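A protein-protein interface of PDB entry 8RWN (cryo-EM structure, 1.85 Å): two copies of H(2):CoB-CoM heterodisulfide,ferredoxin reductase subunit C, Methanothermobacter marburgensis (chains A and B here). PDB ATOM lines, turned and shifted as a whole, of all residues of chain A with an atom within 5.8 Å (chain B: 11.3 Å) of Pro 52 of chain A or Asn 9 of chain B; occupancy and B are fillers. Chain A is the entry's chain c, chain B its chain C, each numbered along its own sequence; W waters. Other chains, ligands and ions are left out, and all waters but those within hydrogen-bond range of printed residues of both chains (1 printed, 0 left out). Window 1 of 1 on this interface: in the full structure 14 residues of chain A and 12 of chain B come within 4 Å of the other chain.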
ATOM      1  N   SER A  47     -29.735  26.779   2.981  1.00  0.00           N
ATOM      2  CA  SER A  47     -29.811  27.896   2.046  1.00  0.00           C
ATOM      3  C   SER A  47     -28.474  28.612   1.924  1.00  0.00           C
ATOM      4  O   SER A  47     -28.151  29.129   0.851  1.00  0.00           O
ATOM      5  CB  SER A  47     -30.909  28.878   2.460  1.00  0.00           C
ATOM      6  OG  SER A  47     -30.701  29.371   3.769  1.00  0.00           O
ATOM      7  N   GLY A  48     -27.684  28.639   2.998  1.00  0.00           N
ATOM      8  CA  GLY A  48     -26.369  29.250   2.932  1.00  0.00           C
ATOM      9  C   GLY A  48     -25.445  28.598   1.926  1.00  0.00           C
ATOM     10  O   GLY A  48     -24.523  29.252   1.431  1.00  0.00           O
ATOM     11  N   ARG A  49     -25.673  27.325   1.606  1.00  0.00           N
ATOM     12  CA  ARG A  49     -24.823  26.597   0.672  1.00  0.00           C
ATOM     13  C   ARG A  49     -25.075  26.956  -0.784  1.00  0.00           C
ATOM     14  O   ARG A  49     -24.235  26.636  -1.627  1.00  0.00           O
ATOM     15  CB  ARG A  49     -25.019  25.085   0.832  1.00  0.00           C
ATOM     16  CG  ARG A  49     -24.744  24.550   2.213  1.00  0.00           C
ATOM     17  CD  ARG A  49     -24.279  23.100   2.165  1.00  0.00           C
ATOM     18  NE  ARG A  49     -25.363  22.170   1.869  1.00  0.00           N
ATOM     19  CZ  ARG A  49     -26.304  21.815   2.734  1.00  0.00           C
ATOM     20  NH1 ARG A  49     -26.341  22.310   3.960  1.00  0.00           N
ATOM     21  NH2 ARG A  49     -27.231  20.939   2.360  1.00  0.00           N
ATOM     22  N   ARG A  50     -26.203  27.593  -1.102  1.00  0.00           N
ATOM     23  CA  ARG A  50     -26.575  27.846  -2.484  1.00  0.00           C
ATOM     24  C   ARG A  50     -27.017  29.279  -2.743  1.00  0.00           C
ATOM     25  O   ARG A  50     -27.410  29.589  -3.872  1.00  0.00           O
ATOM     26  CB  ARG A  50     -27.693  26.883  -2.913  1.00  0.00           C
ATOM     27  CG  ARG A  50     -29.014  27.101  -2.201  1.00  0.00           C
ATOM     28  CD  ARG A  50     -29.806  25.807  -2.100  1.00  0.00           C
ATOM     29  NE  ARG A  50     -29.288  24.935  -1.052  1.00  0.00           N
ATOM     30  CZ  ARG A  50     -29.072  23.631  -1.180  1.00  0.00           C
ATOM     31  NH1 ARG A  50     -29.341  22.986  -2.304  1.00  0.00           N
ATOM     32  NH2 ARG A  50     -28.577  22.953  -0.148  1.00  0.00           N
ATOM     33  N   THR A  51     -26.974  30.147  -1.747  1.00  0.00           N
ATOM     34  CA  THR A  51     -27.300  31.555  -1.911  1.00  0.00           C
ATOM     35  C   THR A  51     -26.298  32.384  -1.117  1.00  0.00           C
ATOM     36  O   THR A  51     -25.462  31.822  -0.399  1.00  0.00           O
ATOM     37  CB  THR A  51     -28.726  31.860  -1.439  1.00  0.00           C
ATOM     38  OG1 THR A  51     -28.775  31.842  -0.009  1.00  0.00           O
ATOM     39  CG2 THR A  51     -29.717  30.843  -1.985  1.00  0.00           C
ATOM     40  N   PRO A  52     -26.340  33.711  -1.220  1.00  0.00           N
ATOM     41  CA  PRO A  52     -25.495  34.560  -0.371  1.00  0.00           C
ATOM     42  C   PRO A  52     -25.989  34.713   1.059  1.00  0.00           C
ATOM     43  O   PRO A  52     -25.393  35.479   1.821  1.00  0.00           O
ATOM     44  CB  PRO A  52     -25.527  35.916  -1.098  1.00  0.00           C
ATOM     45  CG  PRO A  52     -26.131  35.650  -2.442  1.00  0.00           C
ATOM     46  CD  PRO A  52     -27.034  34.493  -2.253  1.00  0.00           C
ATOM     47  N   TYR A  53     -27.055  34.022   1.441  1.00  0.00           N
ATOM     48  CA  TYR A  53     -27.616  34.160   2.780  1.00  0.00           C
ATOM     49  C   TYR A  53     -26.645  33.619   3.826  1.00  0.00           C
ATOM     50  O   TYR A  53     -26.215  32.466   3.740  1.00  0.00           O
ATOM     51  CB  TYR A  53     -28.948  33.419   2.848  1.00  0.00           C
ATOM     52  CG  TYR A  53     -29.567  33.386   4.218  1.00  0.00           C
ATOM     53  CD1 TYR A  53     -29.934  34.557   4.855  1.00  0.00           C
ATOM     54  CD2 TYR A  53     -29.793  32.183   4.866  1.00  0.00           C
ATOM     55  CE1 TYR A  53     -30.507  34.533   6.109  1.00  0.00           C
ATOM     56  CE2 TYR A  53     -30.366  32.146   6.114  1.00  0.00           C
ATOM     57  CZ  TYR A  53     -30.719  33.324   6.733  1.00  0.00           C
ATOM     58  OH  TYR A  53     -31.291  33.292   7.982  1.00  0.00           O
ATOM     59  N   ARG A  54     -26.311  34.449   4.815  1.00  0.00           N
ATOM     60  CA  ARG A  54     -25.406  34.075   5.906  1.00  0.00           C
ATOM     61  C   ARG A  54     -26.101  34.389   7.230  1.00  0.00           C
ATOM     62  O   ARG A  54     -26.116  35.539   7.674  1.00  0.00           O
ATOM     63  CB  ARG A  54     -24.070  34.809   5.797  1.00  0.00           C
ATOM     64  CG  ARG A  54     -23.363  34.644   4.455  1.00  0.00           C
ATOM     65  CD  ARG A  54     -22.762  33.258   4.302  1.00  0.00           C
ATOM     66  NE  ARG A  54     -22.055  33.117   3.034  1.00  0.00           N
ATOM     67  CZ  ARG A  54     -22.629  32.805   1.880  1.00  0.00           C
ATOM     68  NH1 ARG A  54     -23.920  32.531   1.801  1.00  0.00           N
ATOM     69  NH2 ARG A  54     -21.886  32.765   0.778  1.00  0.00           N
ATOM     70  N   THR A  75     -31.617  38.411   0.844  1.00  0.00           N
ATOM     71  CA  THR A  75     -31.232  37.107   1.366  1.00  0.00           C
ATOM     72  C   THR A  75     -31.976  36.769   2.649  1.00  0.00           C
ATOM     73  O   THR A  75     -32.059  35.591   3.008  1.00  0.00           O
ATOM     74  CB  THR A  75     -29.719  37.034   1.615  1.00  0.00           C
ATOM     75  OG1 THR A  75     -29.337  37.986   2.613  1.00  0.00           O
ATOM     76  CG2 THR A  75     -28.943  37.298   0.332  1.00  0.00           C
ATOM     77  N   MET B   1     -35.182  38.520  -9.397  1.00  0.00           N
ATOM     78  CA  MET B   1     -34.036  37.667  -9.823  1.00  0.00           C
ATOM     79  C   MET B   1     -33.754  36.652  -8.722  1.00  0.00           C
ATOM     80  O   MET B   1     -33.711  37.005  -7.544  1.00  0.00           O
ATOM     81  CB  MET B   1     -32.796  38.525 -10.102  1.00  0.00           C
ATOM     82  CG  MET B   1     -31.533  37.758 -10.519  1.00  0.00           C
ATOM     83  SD  MET B   1     -31.847  36.211 -11.398  1.00  0.00           S
ATOM     84  CE  MET B   1     -30.344  35.285 -11.070  1.00  0.00           C
ATOM     85  N   THR B   2     -33.574  35.391  -9.100  1.00  0.00           N
ATOM     86  CA  THR B   2     -33.276  34.361  -8.116  1.00  0.00           C
ATOM     87  C   THR B   2     -31.928  34.633  -7.461  1.00  0.00           C
ATOM     88  O   THR B   2     -31.032  35.238  -8.052  1.00  0.00           O
ATOM     89  CB  THR B   2     -33.266  32.975  -8.763  1.00  0.00           C
ATOM     90  OG1 THR B   2     -32.985  31.982  -7.769  1.00  0.00           O
ATOM     91  CG2 THR B   2     -32.214  32.891  -9.861  1.00  0.00           C
ATOM     92  N   LEU B   3     -31.797  34.196  -6.217  1.00  0.00           N
ATOM     93  CA  LEU B   3     -30.522  34.252  -5.523  1.00  0.00           C
ATOM     94  C   LEU B   3     -29.727  32.961  -5.663  1.00  0.00           C
ATOM     95  O   LEU B   3     -28.617  32.874  -5.131  1.00  0.00           O
ATOM     96  CB  LEU B   3     -30.749  34.574  -4.045  1.00  0.00           C
ATOM     97  CG  LEU B   3     -31.289  35.982  -3.780  1.00  0.00           C
ATOM     98  CD1 LEU B   3     -31.917  36.083  -2.401  1.00  0.00           C
ATOM     99  CD2 LEU B   3     -30.197  37.023  -3.945  1.00  0.00           C
ATOM    100  N   LEU B   4     -30.260  31.969  -6.374  1.00  0.00           N
ATOM    101  CA  LEU B   4     -29.594  30.679  -6.478  1.00  0.00           C
ATOM    102  C   LEU B   4     -28.252  30.828  -7.182  1.00  0.00           C
ATOM    103  O   LEU B   4     -28.153  31.461  -8.237  1.00  0.00           O
ATOM    104  CB  LEU B   4     -30.470  29.680  -7.232  1.00  0.00           C
ATOM    105  CG  LEU B   4     -29.848  28.295  -7.452  1.00  0.00           C
ATOM    106  CD1 LEU B   4     -29.651  27.563  -6.130  1.00  0.00           C
ATOM    107  CD2 LEU B   4     -30.696  27.461  -8.399  1.00  0.00           C
ATOM    108  N   GLN B   5     -27.219  30.242  -6.586  1.00  0.00           N
ATOM    109  CA  GLN B   5     -25.894  30.205  -7.194  1.00  0.00           C
ATOM    110  C   GLN B   5     -25.142  29.068  -6.517  1.00  0.00           C
ATOM    111  O   GLN B   5     -24.760  29.189  -5.350  1.00  0.00           O
ATOM    112  CB  GLN B   5     -25.175  31.534  -7.027  1.00  0.00           C
ATOM    113  CG  GLN B   5     -24.491  32.020  -8.293  1.00  0.00           C
ATOM    114  CD  GLN B   5     -23.542  30.993  -8.874  1.00  0.00           C
ATOM    115  OE1 GLN B   5     -23.040  30.122  -8.167  1.00  0.00           O
ATOM    116  NE2 GLN B   5     -23.296  31.088 -10.173  1.00  0.00           N
ATOM    117  N   ARG B   6     -24.942  27.977  -7.246  1.00  0.00           N
ATOM    118  CA  ARG B   6     -24.529  26.717  -6.647  1.00  0.00           C
ATOM    119  C   ARG B   6     -23.022  26.578  -6.480  1.00  0.00           C
ATOM    120  O   ARG B   6     -22.581  25.691  -5.742  1.00  0.00           O
ATOM    121  CB  ARG B   6     -25.068  25.555  -7.491  1.00  0.00           C
ATOM    122  CG  ARG B   6     -26.592  25.530  -7.574  1.00  0.00           C
ATOM    123  CD  ARG B   6     -27.103  24.891  -8.860  1.00  0.00           C
ATOM    124  NE  ARG B   6     -27.203  23.439  -8.763  1.00  0.00           N
ATOM    125  CZ  ARG B   6     -26.445  22.576  -9.429  1.00  0.00           C
ATOM    126  NH1 ARG B   6     -25.485  22.977 -10.247  1.00  0.00           N
ATOM    127  NH2 ARG B   6     -26.655  21.273  -9.267  1.00  0.00           N
ATOM    128  N   GLU B   7     -22.221  27.427  -7.124  1.00  0.00           N
ATOM    129  CA  GLU B   7     -20.768  27.347  -7.014  1.00  0.00           C
ATOM    130  C   GLU B   7     -20.143  28.503  -6.251  1.00  0.00           C
ATOM    131  O   GLU B   7     -19.059  28.335  -5.692  1.00  0.00           O
ATOM    132  CB  GLU B   7     -20.119  27.285  -8.405  1.00  0.00           C
ATOM    133  CG  GLU B   7     -20.839  26.410  -9.414  1.00  0.00           C
ATOM    134  CD  GLU B   7     -22.039  27.097 -10.031  1.00  0.00           C
ATOM    135  OE1 GLU B   7     -21.845  28.073 -10.784  1.00  0.00           O
ATOM    136  OE2 GLU B   7     -23.176  26.664  -9.761  1.00  0.00           O
ATOM    137  N   GLU B   8     -20.790  29.665  -6.212  1.00  0.00           N
ATOM    138  CA  GLU B   8     -20.206  30.844  -5.586  1.00  0.00           C
ATOM    139  C   GLU B   8     -20.353  30.858  -4.072  1.00  0.00           C
ATOM    140  O   GLU B   8     -19.703  31.678  -3.416  1.00  0.00           O
ATOM    141  CB  GLU B   8     -20.846  32.111  -6.154  1.00  0.00           C
ATOM    142  CG  GLU B   8     -20.301  32.533  -7.502  1.00  0.00           C
ATOM    143  CD  GLU B   8     -21.268  33.413  -8.268  1.00  0.00           C
ATOM    144  OE1 GLU B   8     -22.025  34.171  -7.626  1.00  0.00           O
ATOM    145  OE2 GLU B   8     -21.275  33.340  -9.515  1.00  0.00           O
ATOM    146  N   ASN B   9     -21.185  29.986  -3.503  1.00  0.00           N
ATOM    147  CA  ASN B   9     -21.536  30.059  -2.089  1.00  0.00           C
ATOM    148  C   ASN B   9     -21.047  28.852  -1.297  1.00  0.00           C
ATOM    149  O   ASN B   9     -21.529  28.608  -0.188  1.00  0.00           O
ATOM    150  CB  ASN B   9     -23.048  30.217  -1.943  1.00  0.00           C
ATOM    151  CG  ASN B   9     -23.536  31.549  -2.468  1.00  0.00           C
ATOM    152  OD1 ASN B   9     -23.214  32.597  -1.915  1.00  0.00           O
ATOM    153  ND2 ASN B   9     -24.318  31.517  -3.538  1.00  0.00           N
ATOM    154  N   ILE B  10     -20.097  28.094  -1.837  1.00  0.00           N
ATOM    155  CA  ILE B  10     -19.528  26.953  -1.135  1.00  0.00           C
ATOM    156  C   ILE B  10     -18.103  26.751  -1.629  1.00  0.00           C
ATOM    157  O   ILE B  10     -17.799  26.974  -2.802  1.00  0.00           O
ATOM    158  CB  ILE B  10     -20.376  25.676  -1.341  1.00  0.00           C
ATOM    159  CG1 ILE B  10     -19.953  24.589  -0.354  1.00  0.00           C
ATOM    160  CG2 ILE B  10     -20.254  25.168  -2.778  1.00  0.00           C
ATOM    161  CD1 ILE B  10     -21.004  23.526  -0.130  1.00  0.00           C
ATOM    162  N   ILE B  11     -17.228  26.322  -0.725  1.00  0.00           N
ATOM    163  CA  ILE B  11     -15.834  26.035  -1.049  1.00  0.00           C
ATOM    164  C   ILE B  11     -15.608  24.537  -0.901  1.00  0.00           C
ATOM    165  O   ILE B  11     -15.849  23.966   0.169  1.00  0.00           O
ATOM    166  CB  ILE B  11     -14.862  26.826  -0.159  1.00  0.00           C
ATOM    167  CG1 ILE B  11     -15.192  28.320  -0.188  1.00  0.00           C
ATOM    168  CG2 ILE B  11     -13.435  26.595  -0.622  1.00  0.00           C
ATOM    169  CD1 ILE B  11     -14.369  29.153   0.776  1.00  0.00           C
ATOM    170  N   ARG B  12     -15.144  23.906  -1.975  1.00  0.00           N
ATOM    171  CA  ARG B  12     -14.740  22.507  -1.987  1.00  0.00           C
ATOM    172  C   ARG B  12     -13.325  22.420  -2.544  1.00  0.00           C
ATOM    173  O   ARG B  12     -12.742  23.420  -2.972  1.00  0.00           O
ATOM    174  CB  ARG B  12     -15.705  21.652  -2.820  1.00  0.00           C
ATOM    175  CG  ARG B  12     -17.138  21.648  -2.318  1.00  0.00           C
ATOM    176  CD  ARG B  12     -17.842  20.342  -2.666  1.00  0.00           C
ATOM    177  NE  ARG B  12     -19.242  20.346  -2.261  1.00  0.00           N
ATOM    178  CZ  ARG B  12     -20.200  21.010  -2.892  1.00  0.00           C
ATOM    179  NH1 ARG B  12     -19.945  21.736  -3.967  1.00  0.00           N
ATOM    180  NH2 ARG B  12     -21.445  20.947  -2.431  1.00  0.00           N
ATOM    181  N   ASN B  15     -12.182  24.227  -5.793  1.00  0.00           N
ATOM    182  CA  ASN B  15     -11.851  25.643  -5.827  1.00  0.00           C
ATOM    183  C   ASN B  15     -10.429  25.931  -5.365  1.00  0.00           C
ATOM    184  O   ASN B  15     -10.038  27.100  -5.308  1.00  0.00           O
ATOM    185  CB  ASN B  15     -12.829  26.434  -4.952  1.00  0.00           C
ATOM    186  CG  ASN B  15     -14.271  26.063  -5.205  1.00  0.00           C
ATOM    187  OD1 ASN B  15     -14.885  25.340  -4.422  1.00  0.00           O
ATOM    188  ND2 ASN B  15     -14.823  26.557  -6.305  1.00  0.00           N
ATOM    189  N   LEU B  66      -7.083  29.634  -3.087  1.00  0.00           N
ATOM    190  CA  LEU B  66      -8.166  29.988  -4.005  1.00  0.00           C
ATOM    191  C   LEU B  66      -7.611  30.881  -5.118  1.00  0.00           C
ATOM    192  O   LEU B  66      -7.872  32.081  -5.201  1.00  0.00           O
ATOM    193  CB  LEU B  66      -9.306  30.659  -3.250  1.00  0.00           C
ATOM    194  CG  LEU B  66      -9.859  29.850  -2.073  1.00  0.00           C
ATOM    195  CD1 LEU B  66     -10.799  30.691  -1.223  1.00  0.00           C
ATOM    196  CD2 LEU B  66     -10.560  28.593  -2.572  1.00  0.00           C
ATOM    197  N   GLU B  69     -10.095  32.710  -7.532  1.00  0.00           N
ATOM    198  CA  GLU B  69     -10.748  33.812  -6.840  1.00  0.00           C
ATOM    199  C   GLU B  69      -9.818  35.011  -6.689  1.00  0.00           C
ATOM    200  O   GLU B  69     -10.266  36.159  -6.765  1.00  0.00           O
ATOM    201  CB  GLU B  69     -11.243  33.347  -5.473  1.00  0.00           C
ATOM    202  CG  GLU B  69     -12.489  34.054  -5.006  1.00  0.00           C
ATOM    203  CD  GLU B  69     -13.133  33.362  -3.826  1.00  0.00           C
ATOM    204  OE1 GLU B  69     -13.546  34.063  -2.880  1.00  0.00           O
ATOM    205  OE2 GLU B  69     -13.230  32.118  -3.849  1.00  0.00           O
HETATM  206  O   HOH W   1     -21.797  29.887   2.304  1.00  0.00           O
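The guanidinium group of Arg 54 of chain A sits at hydrogen-bond distance from the side-chain amide oxygen of Asn 9 of chain B. The side-chain amide oxygen (OD1) of Asn 9 of chain B sits close to the backbone carbonyl oxygen (O) of Thr 51 of chain A (2.8 Å). The backbone carbonyl oxygen of Arg 50 of chain A lies within hydrogen-bond range of the backbone NH of Gln 5 of chain B, at 2.8 Å. The backbone carbonyl oxygen of Asn 9 of chain B sits close to the backbone carbonyl oxygen of Gly 48 of chain A (3.5 Å). The side-chain amide oxygen (OD1) of Asn 9 of chain B lies close to the backbone nitrogen (N) of Pro 52 of chain A, 3.4 Å away.
O of Gln 5 of chain B is in hydrogen-bond range of ND2 of Asn 9 of chain B. The backbone NH (N) of Tyr 53 of chain A lies close to the side-chain hydroxyl (OG1) of Thr 51 of chain A, at 3.1 Å. The backbone carbonyl oxygen (O) of Ser 47 of chain A lies within hydrogen-bond range of the side-chain hydroxyl (OG1) of Thr 51 of chain A. The guanidinium group (NH1) of Arg 54 of chain A lies within hydrogen-bond range of the backbone carbonyl oxygen (O) of Gly 48 of chain A (3.4 Å). The backbone carbonyl oxygen of Pro 52 of chain A lies close to the guanidinium group of Arg 54 of chain A, at 3.3 Å. The side-chain amide oxygen of Gln 5 of chain B sits at hydrogen-bond distance from the backbone NH of Glu 8 of chain B (3.0 Å).
Among the printed residues, pairs that only touch across the chains: Arg 49 of chain A with Asn 9 of chain B (3.6 Å), Arg 49 of chain A with Ile 10 of chain B (3.99 Å), Arg 50 of chain A with Leu 3 of chain B (3.7 Å), Arg 50 of chain A with Leu 4 of chain B (3.6 Å), Arg 50 of chain A with Asn 9 of chain B (3.6 Å), Thr 51 of chain A with Leu 3 of chain B (3.7 Å), Pro 52 of chain A with Leu 3 of chain B (3.7 Å) and Thr 75 of chain A with Leu 3 of chain B (3.96 Å).
Pro 52 of chain A touches two residues of chain B. Asn 9 of chain B touches just these residues of chain A: Gly 48 (3.5 Å), Arg 49 (3.6 Å), Arg 50 (3.6 Å), Thr 51 (2.8 Å), Pro 52 (3.4 Å) and Arg 54 (3.0 Å). Gly 48 of chain A touches just one residue of chain B: Asn 9. Of the printed residues of chain A, Leu 4 of chain B touches Arg 50 (3.6 Å). Of the printed residues of chain A, Gln 5 of chain B touches Arg 50. Printed residues of chain A within 4 Å of Ile 10 of chain B: Arg 49. Glu 69 of chain B touches none of the printed residues of chain A. The nearest residue of chain B that does not touch Pro 52 of chain A is Leu 4 of chain B (5.8 Å).
Of the 15 printed residues of chain B, 5 touch a printed residue of chain A. Hydrophobic or aromatic side chains of chain B within 4 Å of the printed part of chain A: Leu 3, Leu 4 and Ile 10. Printed residues of chain A that touch a printed residue of chain B: Gly 48, Arg 49, Arg 50, Thr 51, Pro 52, Arg 54 and Thr 75. Along chain A the printed residues that touch a printed residue of chain B span positions 48 to 75. Among the printed residues, no Asp or Glu carboxylate lies within 4 Å of a Lys or Arg side-chain nitrogen of the other chain.
No position is printed for both chains.
Water W1 lies within hydrogen-bond range of the backbone carbonyl oxygen (O) of Asn 9 of chain B (2.8 Å), the backbone carbonyl oxygen (O) of Gly 48 of chain A (2.9 Å) and the guanidinium group (NH2) of Arg 54 of chain A (3.3 Å).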
